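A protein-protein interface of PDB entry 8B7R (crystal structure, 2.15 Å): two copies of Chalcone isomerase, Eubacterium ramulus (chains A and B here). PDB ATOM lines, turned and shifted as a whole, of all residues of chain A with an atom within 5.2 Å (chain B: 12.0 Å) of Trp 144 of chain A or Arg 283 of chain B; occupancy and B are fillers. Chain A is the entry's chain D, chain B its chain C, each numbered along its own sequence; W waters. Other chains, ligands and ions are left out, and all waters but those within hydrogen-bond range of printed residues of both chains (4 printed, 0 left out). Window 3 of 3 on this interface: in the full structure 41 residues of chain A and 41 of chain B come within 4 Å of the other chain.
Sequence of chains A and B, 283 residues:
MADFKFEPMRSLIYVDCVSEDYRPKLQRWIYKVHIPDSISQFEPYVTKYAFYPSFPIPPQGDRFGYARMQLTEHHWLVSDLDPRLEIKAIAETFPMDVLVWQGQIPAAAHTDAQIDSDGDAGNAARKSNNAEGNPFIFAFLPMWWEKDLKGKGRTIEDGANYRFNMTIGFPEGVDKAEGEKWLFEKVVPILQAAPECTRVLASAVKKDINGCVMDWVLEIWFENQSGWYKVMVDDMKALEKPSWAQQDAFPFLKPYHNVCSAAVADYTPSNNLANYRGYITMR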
ATOM      1  N   PRO A   8       1.264 -21.619 -10.037  1.00  0.00           N
ATOM      2  CA  PRO A   8       1.311 -20.276  -9.458  1.00  0.00           C
ATOM      3  C   PRO A   8       0.015 -19.990  -8.696  1.00  0.00           C
ATOM      4  O   PRO A   8      -1.080 -20.161  -9.226  1.00  0.00           O
ATOM      5  CB  PRO A   8       1.508 -19.349 -10.661  1.00  0.00           C
ATOM      6  CG  PRO A   8       0.903 -20.147 -11.817  1.00  0.00           C
ATOM      7  CD  PRO A   8       1.238 -21.594 -11.516  1.00  0.00           C
ATOM      8  N   ARG A  10      -1.594 -17.496  -5.101  1.00  0.00           N
ATOM      9  CA  ARG A  10      -1.522 -16.585  -3.975  1.00  0.00           C
ATOM     10  C   ARG A  10      -2.288 -17.235  -2.838  1.00  0.00           C
ATOM     11  O   ARG A  10      -3.382 -17.750  -3.071  1.00  0.00           O
ATOM     12  CB  ARG A  10      -2.161 -15.251  -4.388  1.00  0.00           C
ATOM     13  CG  ARG A  10      -2.123 -14.162  -3.339  1.00  0.00           C
ATOM     14  CD  ARG A  10      -2.982 -12.987  -3.790  1.00  0.00           C
ATOM     15  NE  ARG A  10      -2.853 -11.831  -2.904  1.00  0.00           N
ATOM     16  CZ  ARG A  10      -3.858 -11.045  -2.497  1.00  0.00           C
ATOM     17  NH1 ARG A  10      -5.076 -11.209  -2.999  1.00  0.00           N
ATOM     18  NH2 ARG A  10      -3.618 -10.096  -1.599  1.00  0.00           N
ATOM     19  N   GLU A  73       0.606 -13.296   3.430  1.00  0.00           N
ATOM     20  CA  GLU A  73       0.420 -13.511   1.999  1.00  0.00           C
ATOM     21  C   GLU A  73       1.661 -14.180   1.407  1.00  0.00           C
ATOM     22  O   GLU A  73       2.769 -13.674   1.585  1.00  0.00           O
ATOM     23  CB  GLU A  73       0.144 -12.165   1.328  1.00  0.00           C
ATOM     24  CG  GLU A  73      -0.056 -12.214  -0.172  1.00  0.00           C
ATOM     25  CD  GLU A  73       0.186 -10.860  -0.821  1.00  0.00           C
ATOM     26  OE1 GLU A  73       1.354 -10.324  -0.677  1.00  0.00           O
ATOM     27  OE2 GLU A  73      -0.761 -10.324  -1.490  1.00  0.00           O
ATOM     28  N   HIS A  75       3.145 -15.871  -2.426  1.00  0.00           N
ATOM     29  CA  HIS A  75       2.992 -16.214  -3.835  1.00  0.00           C
ATOM     30  C   HIS A  75       3.919 -17.394  -4.133  1.00  0.00           C
ATOM     31  O   HIS A  75       5.135 -17.270  -4.027  1.00  0.00           O
ATOM     32  CB  HIS A  75       3.253 -14.998  -4.721  1.00  0.00           C
ATOM     33  CG  HIS A  75       2.214 -13.907  -4.660  1.00  0.00           C
ATOM     34  ND1 HIS A  75       2.087 -13.025  -3.612  1.00  0.00           N
ATOM     35  CD2 HIS A  75       1.312 -13.508  -5.610  1.00  0.00           C
ATOM     36  CE1 HIS A  75       1.118 -12.139  -3.917  1.00  0.00           C
ATOM     37  NE2 HIS A  75       0.621 -12.408  -5.138  1.00  0.00           N
ATOM     38  N   PRO A 142      -5.873 -18.386  -7.160  1.00  0.00           N
ATOM     39  CA  PRO A 142      -5.058 -17.987  -8.306  1.00  0.00           C
ATOM     40  C   PRO A 142      -4.423 -16.630  -8.002  1.00  0.00           C
ATOM     41  O   PRO A 142      -4.917 -15.896  -7.141  1.00  0.00           O
ATOM     42  CB  PRO A 142      -6.086 -17.915  -9.428  1.00  0.00           C
ATOM     43  CG  PRO A 142      -7.379 -17.604  -8.721  1.00  0.00           C
ATOM     44  CD  PRO A 142      -7.314 -18.377  -7.433  1.00  0.00           C
ATOM     45  N   MET A 143      -3.342 -16.294  -8.714  1.00  0.00           N
ATOM     46  CA  MET A 143      -2.610 -15.064  -8.450  1.00  0.00           C
ATOM     47  C   MET A 143      -3.400 -13.833  -8.881  1.00  0.00           C
ATOM     48  O   MET A 143      -3.060 -12.732  -8.431  1.00  0.00           O
ATOM     49  CB  MET A 143      -1.269 -15.044  -9.170  1.00  0.00           C
ATOM     50  CG  MET A 143      -0.250 -15.929  -8.540  1.00  0.00           C
ATOM     51  SD  MET A 143       1.372 -15.533  -9.195  1.00  0.00           S
ATOM     52  CE  MET A 143       2.401 -16.633  -8.215  1.00  0.00           C
ATOM     53  N   TRP A 144      -4.414 -14.016  -9.746  1.00  0.00           N
ATOM     54  CA  TRP A 144      -5.235 -12.932 -10.267  1.00  0.00           C
ATOM     55  C   TRP A 144      -6.696 -13.145  -9.877  1.00  0.00           C
ATOM     56  O   TRP A 144      -7.225 -14.265  -9.912  1.00  0.00           O
ATOM     57  CB  TRP A 144      -5.071 -12.803 -11.777  1.00  0.00           C
ATOM     58  CG  TRP A 144      -3.640 -12.637 -12.179  1.00  0.00           C
ATOM     59  CD1 TRP A 144      -2.933 -11.466 -12.277  1.00  0.00           C
ATOM     60  CD2 TRP A 144      -2.694 -13.705 -12.395  1.00  0.00           C
ATOM     61  NE1 TRP A 144      -1.617 -11.741 -12.567  1.00  0.00           N
ATOM     62  CE2 TRP A 144      -1.441 -13.102 -12.645  1.00  0.00           C
ATOM     63  CE3 TRP A 144      -2.780 -15.102 -12.409  1.00  0.00           C
ATOM     64  CZ2 TRP A 144      -0.307 -13.854 -12.946  1.00  0.00           C
ATOM     65  CZ3 TRP A 144      -1.658 -15.846 -12.723  1.00  0.00           C
ATOM     66  CH2 TRP A 144      -0.434 -15.227 -12.954  1.00  0.00           C
ATOM     67  N   TRP A 145      -7.340 -12.038  -9.476  1.00  0.00           N
ATOM     68  CA  TRP A 145      -8.725 -12.086  -9.060  1.00  0.00           C
ATOM     69  C   TRP A 145      -9.562 -12.595 -10.222  1.00  0.00           C
ATOM     70  O   TRP A 145      -9.329 -12.171 -11.369  1.00  0.00           O
ATOM     71  CB  TRP A 145      -9.193 -10.689  -8.640  1.00  0.00           C
ATOM     72  CG  TRP A 145      -8.591 -10.192  -7.370  1.00  0.00           C
ATOM     73  CD1 TRP A 145      -7.607  -9.253  -7.231  1.00  0.00           C
ATOM     74  CD2 TRP A 145      -8.981 -10.561  -6.044  1.00  0.00           C
ATOM     75  NE1 TRP A 145      -7.348  -9.036  -5.896  1.00  0.00           N
ATOM     76  CE2 TRP A 145      -8.181  -9.820  -5.153  1.00  0.00           C
ATOM     77  CE3 TRP A 145      -9.939 -11.432  -5.521  1.00  0.00           C
ATOM     78  CZ2 TRP A 145      -8.298  -9.937  -3.770  1.00  0.00           C
ATOM     79  CZ3 TRP A 145     -10.055 -11.552  -4.154  1.00  0.00           C
ATOM     80  CH2 TRP A 145      -9.252 -10.803  -3.290  1.00  0.00           C
ATOM     81  N   GLU A 146     -10.542 -13.458  -9.919  1.00  0.00           N
ATOM     82  CA  GLU A 146     -11.349 -14.073 -10.961  1.00  0.00           C
ATOM     83  C   GLU A 146     -12.472 -13.141 -11.394  1.00  0.00           C
ATOM     84  O   GLU A 146     -12.841 -13.116 -12.565  1.00  0.00           O
ATOM     85  CB  GLU A 146     -11.885 -15.416 -10.484  1.00  0.00           C
ATOM     86  CG  GLU A 146     -10.785 -16.463 -10.426  1.00  0.00           C
ATOM     87  CD  GLU A 146     -11.187 -17.784  -9.796  1.00  0.00           C
ATOM     88  OE1 GLU A 146     -12.168 -17.800  -9.013  1.00  0.00           O
ATOM     89  OE2 GLU A 146     -10.535 -18.797 -10.134  1.00  0.00           O
ATOM     90  N   ARG A 163      -9.042  -1.513   2.818  1.00  0.00           N
ATOM     91  CA  ARG A 163      -9.260  -2.715   2.019  1.00  0.00           C
ATOM     92  C   ARG A 163      -9.735  -3.848   2.922  1.00  0.00           C
ATOM     93  O   ARG A 163      -8.972  -4.369   3.715  1.00  0.00           O
ATOM     94  CB  ARG A 163      -7.974  -3.094   1.270  1.00  0.00           C
ATOM     95  CG  ARG A 163      -7.464  -1.967   0.380  1.00  0.00           C
ATOM     96  CD  ARG A 163      -6.138  -2.159  -0.310  1.00  0.00           C
ATOM     97  NE  ARG A 163      -6.140  -3.259  -1.234  1.00  0.00           N
ATOM     98  CZ  ARG A 163      -5.280  -3.423  -2.241  1.00  0.00           C
ATOM     99  NH1 ARG A 163      -4.425  -2.471  -2.611  1.00  0.00           N
ATOM    100  NH2 ARG A 163      -5.333  -4.581  -2.876  1.00  0.00           N
ATOM    101  N   SER A 203     -12.573 -14.173  -5.784  1.00  0.00           N
ATOM    102  CA  SER A 203     -12.012 -15.395  -6.309  1.00  0.00           C
ATOM    103  C   SER A 203     -12.601 -16.564  -5.525  1.00  0.00           C
ATOM    104  O   SER A 203     -12.878 -16.458  -4.320  1.00  0.00           O
ATOM    105  CB  SER A 203     -10.504 -15.412  -6.250  1.00  0.00           C
ATOM    106  OG  SER A 203      -9.917 -14.544  -7.228  1.00  0.00           O
ATOM    107  N   GLU A 219     -12.503  -9.046  -1.716  1.00  0.00           N
ATOM    108  CA  GLU A 219     -11.952  -7.823  -1.182  1.00  0.00           C
ATOM    109  C   GLU A 219     -12.877  -6.678  -1.569  1.00  0.00           C
ATOM    110  O   GLU A 219     -13.249  -6.532  -2.737  1.00  0.00           O
ATOM    111  CB  GLU A 219     -10.511  -7.632  -1.633  1.00  0.00           C
ATOM    112  CG  GLU A 219      -9.769  -6.672  -0.724  1.00  0.00           C
ATOM    113  CD  GLU A 219      -8.272  -6.670  -0.925  1.00  0.00           C
ATOM    114  OE1 GLU A 219      -7.614  -7.679  -0.463  1.00  0.00           O
ATOM    115  OE2 GLU A 219      -7.783  -5.719  -1.596  1.00  0.00           O
ATOM    116  N   TYR B 279       6.433   2.764  -2.818  1.00  0.00           N
ATOM    117  CA  TYR B 279       5.083   2.515  -2.331  1.00  0.00           C
ATOM    118  C   TYR B 279       4.458   1.434  -3.213  1.00  0.00           C
ATOM    119  O   TYR B 279       3.696   1.712  -4.160  1.00  0.00           O
ATOM    120  CB  TYR B 279       4.279   3.824  -2.289  1.00  0.00           C
ATOM    121  CG  TYR B 279       2.985   3.772  -1.508  1.00  0.00           C
ATOM    122  CD1 TYR B 279       2.987   3.876  -0.128  1.00  0.00           C
ATOM    123  CD2 TYR B 279       1.750   3.659  -2.143  1.00  0.00           C
ATOM    124  CE1 TYR B 279       1.810   3.859   0.600  1.00  0.00           C
ATOM    125  CE2 TYR B 279       0.567   3.650  -1.431  1.00  0.00           C
ATOM    126  CZ  TYR B 279       0.590   3.729  -0.046  1.00  0.00           C
ATOM    127  OH  TYR B 279      -0.601   3.726   0.700  1.00  0.00           O
ATOM    128  N   ILE B 280       4.861   0.199  -2.922  1.00  0.00           N
ATOM    129  CA  ILE B 280       4.354  -0.980  -3.613  1.00  0.00           C
ATOM    130  C   ILE B 280       2.974  -1.299  -3.037  1.00  0.00           C
ATOM    131  O   ILE B 280       2.817  -1.376  -1.832  1.00  0.00           O
ATOM    132  CB  ILE B 280       5.326  -2.165  -3.431  1.00  0.00           C
ATOM    133  CG1 ILE B 280       6.756  -1.821  -3.869  1.00  0.00           C
ATOM    134  CG2 ILE B 280       4.832  -3.404  -4.158  1.00  0.00           C
ATOM    135  CD1 ILE B 280       6.852  -1.213  -5.263  1.00  0.00           C
ATOM    136  N   THR B 281       1.983  -1.464  -3.911  1.00  0.00           N
ATOM    137  CA  THR B 281       0.613  -1.681  -3.497  1.00  0.00           C
ATOM    138  C   THR B 281       0.227  -3.159  -3.589  1.00  0.00           C
ATOM    139  O   THR B 281       0.657  -3.891  -4.480  1.00  0.00           O
ATOM    140  CB  THR B 281      -0.350  -0.815  -4.315  1.00  0.00           C
ATOM    141  OG1 THR B 281      -0.225  -1.087  -5.722  1.00  0.00           O
ATOM    142  CG2 THR B 281      -0.111   0.645  -4.026  1.00  0.00           C
ATOM    143  N   MET B 282      -0.658  -3.554  -2.663  1.00  0.00           N
ATOM    144  CA  MET B 282      -1.164  -4.908  -2.585  1.00  0.00           C
ATOM    145  C   MET B 282      -2.011  -5.203  -3.825  1.00  0.00           C
ATOM    146  O   MET B 282      -2.723  -4.346  -4.352  1.00  0.00           O
ATOM    147  CB  MET B 282      -1.973  -5.097  -1.294  1.00  0.00           C
ATOM    148  CG  MET B 282      -2.487  -6.523  -1.108  1.00  0.00           C
ATOM    149  SD  MET B 282      -3.247  -6.847   0.499  1.00  0.00           S
ATOM    150  CE  MET B 282      -4.605  -5.680   0.435  1.00  0.00           C
ATOM    151  N   ARG B 283      -1.893  -6.440  -4.291  1.00  0.00           N
ATOM    152  CA  ARG B 283      -2.572  -6.981  -5.456  1.00  0.00           C
ATOM    153  C   ARG B 283      -3.995  -7.477  -5.099  1.00  0.00           C
ATOM    154  O   ARG B 283      -4.509  -7.127  -4.004  1.00  0.00           O
ATOM    155  CB  ARG B 283      -1.718  -8.131  -6.007  1.00  0.00           C
ATOM    156  CG  ARG B 283      -0.305  -7.734  -6.419  1.00  0.00           C
ATOM    157  CD  ARG B 283       0.538  -8.910  -6.939  1.00  0.00           C
ATOM    158  NE  ARG B 283       0.051  -9.405  -8.211  1.00  0.00           N
ATOM    159  CZ  ARG B 283      -0.791 -10.437  -8.341  1.00  0.00           C
ATOM    160  NH1 ARG B 283      -1.037 -11.299  -7.353  1.00  0.00           N
ATOM    161  NH2 ARG B 283      -1.392 -10.611  -9.499  1.00  0.00           N
ATOM    162  OXT ARG B 283      -4.574  -8.180  -5.952  1.00  0.00           O
HETATM  163  O   HOH W   1      -5.798  -8.426  -2.128  1.00  0.00           O
HETATM  164  O   HOH W   2      -4.489 -11.052  -6.428  1.00  0.00           O
HETATM  165  O   HOH W   3       0.120  -8.409  -3.229  1.00  0.00           O
HETATM  166  O   HOH W   4      -1.222  -8.440 -11.586  1.00  0.00           O
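Among the printed residues, pairs that only touch across the chains: Glu 219 of chain A with Met 282 of chain B (3.7 Å) and Arg 10 of chain A with Met 282 of chain B (3.8 Å).
The guanidinium group of Arg 283 of chain B is in hydrogen-bond range of the backbone carbonyl oxygen of Met 143 of chain A. The indole nitrogen (NE1) of Trp 144 of chain A sits close to the guanidinium group (NH2) of Arg 283 of chain B, 3.3 Å away. The chain-end carboxylate (OXT) of Arg 283 of chain B is in hydrogen-bond range of the indole nitrogen (NE1) of Trp 145 of chain A, at 2.9 Å. The chain-end carboxylate (O) of Arg 283 of chain B lies within salt-bridge range of the guanidinium group (NH2) of Arg 163 of chain A (2.9 Å). NH2 of Arg 163 of chain A sits at hydrogen-bond distance from O of Met 282 of chain B (3.0 Å). The guanidinium group (NH2) of Arg 10 of chain A is in salt-bridge range of the chain-end carboxylate (O) of Arg 283 of chain B (3.9 Å). The guanidinium group (NH1) of Arg 283 of chain B lies within hydrogen-bond range of a ring nitrogen (NE2) of His 75 of chain A (3.0 Å).
NE of Arg 163 of chain A is in salt-bridge range of OE2 of Glu 219 of chain A, 3.0 Å away. OE2 of Glu 73 of chain A is in salt-bridge range of NH2 of Arg 10 of chain A, at 2.9 Å.
Printed residues of chain A that touch a printed residue of chain B: Arg 10, His 75, Met 143, Trp 144, Trp 145, Arg 163 and Glu 219. Hydrophobic or aromatic side chains of chain B within 4 Å of the printed part of chain A: Met 282. Among the printed residues, no Asp or Glu carboxylate lies within 4 Å of a Lys or Arg side-chain nitrogen of the other chain.
Of chain B, only Arg 283 comes within 4 Å of Trp 144 of chain A. Of chain A, only Arg 10 (3.9 Å), His 75 (3.0 Å), Met 143 (2.7 Å), Trp 144 (3.3 Å), Trp 145 (2.9 Å) and Arg 163 (2.9 Å) come within 4 Å of Arg 283 of chain B. No residue of chain B comes within 4 Å of Pro 142 of chain A. Met 143 of chain A touches just one residue of chain B: Arg 283 (2.7 Å). Of chain B, only Arg 283 (2.9 Å) comes within 4 Å of Trp 145 of chain A. No residue of chain B comes within 4 Å of Glu 146 of chain A. Printed residues of chain B within 4 Å of His 75 of chain A: Arg 283. Of the printed residues of chain B, Arg 163 of chain A touches Met 282 and Arg 283. Printed residues of chain B within 4 Å of Arg 10 of chain A: Met 282 and Arg 283. Printed residues of chain A within 4 Å of Met 282 of chain B: Arg 10 (3.8 Å), Arg 163 (3.0 Å) and Glu 219 (3.7 Å). Of the printed residues of chain B, Glu 219 of chain A touches Met 282 (3.7 Å). Ile 280 of chain B touches none of the printed residues of chain A. The nearest printed residue of chain B that does not touch Trp 144 of chain A is Met 282 of chain B (10.6 Å).
No position is printed for both chains.
Water W1 lies within hydrogen-bond range of OE1 of Glu 219 of chain A (2.6 Å), O of Arg 283 of chain B (2.6 Å) and NH2 of Arg 10 of chain A (2.8 Å). Water W3 bridges the side-chain carboxylate (OE2) of Glu 73 of chain A and the backbone NH (N) of Arg 283 of chain B. Water W2 lies within hydrogen-bond range of the chain-end carboxylate (OXT) of Arg 283 of chain B, the backbone carbonyl oxygen (O) of Met 143 of chain A and the guanidinium group (NH1) of Arg 10 of chain A. Water W4 bridges the guanidinium group of Arg 283 of chain B (3.0 Å) and the indole nitrogen of Trp 144 of chain A (3.5 Å).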
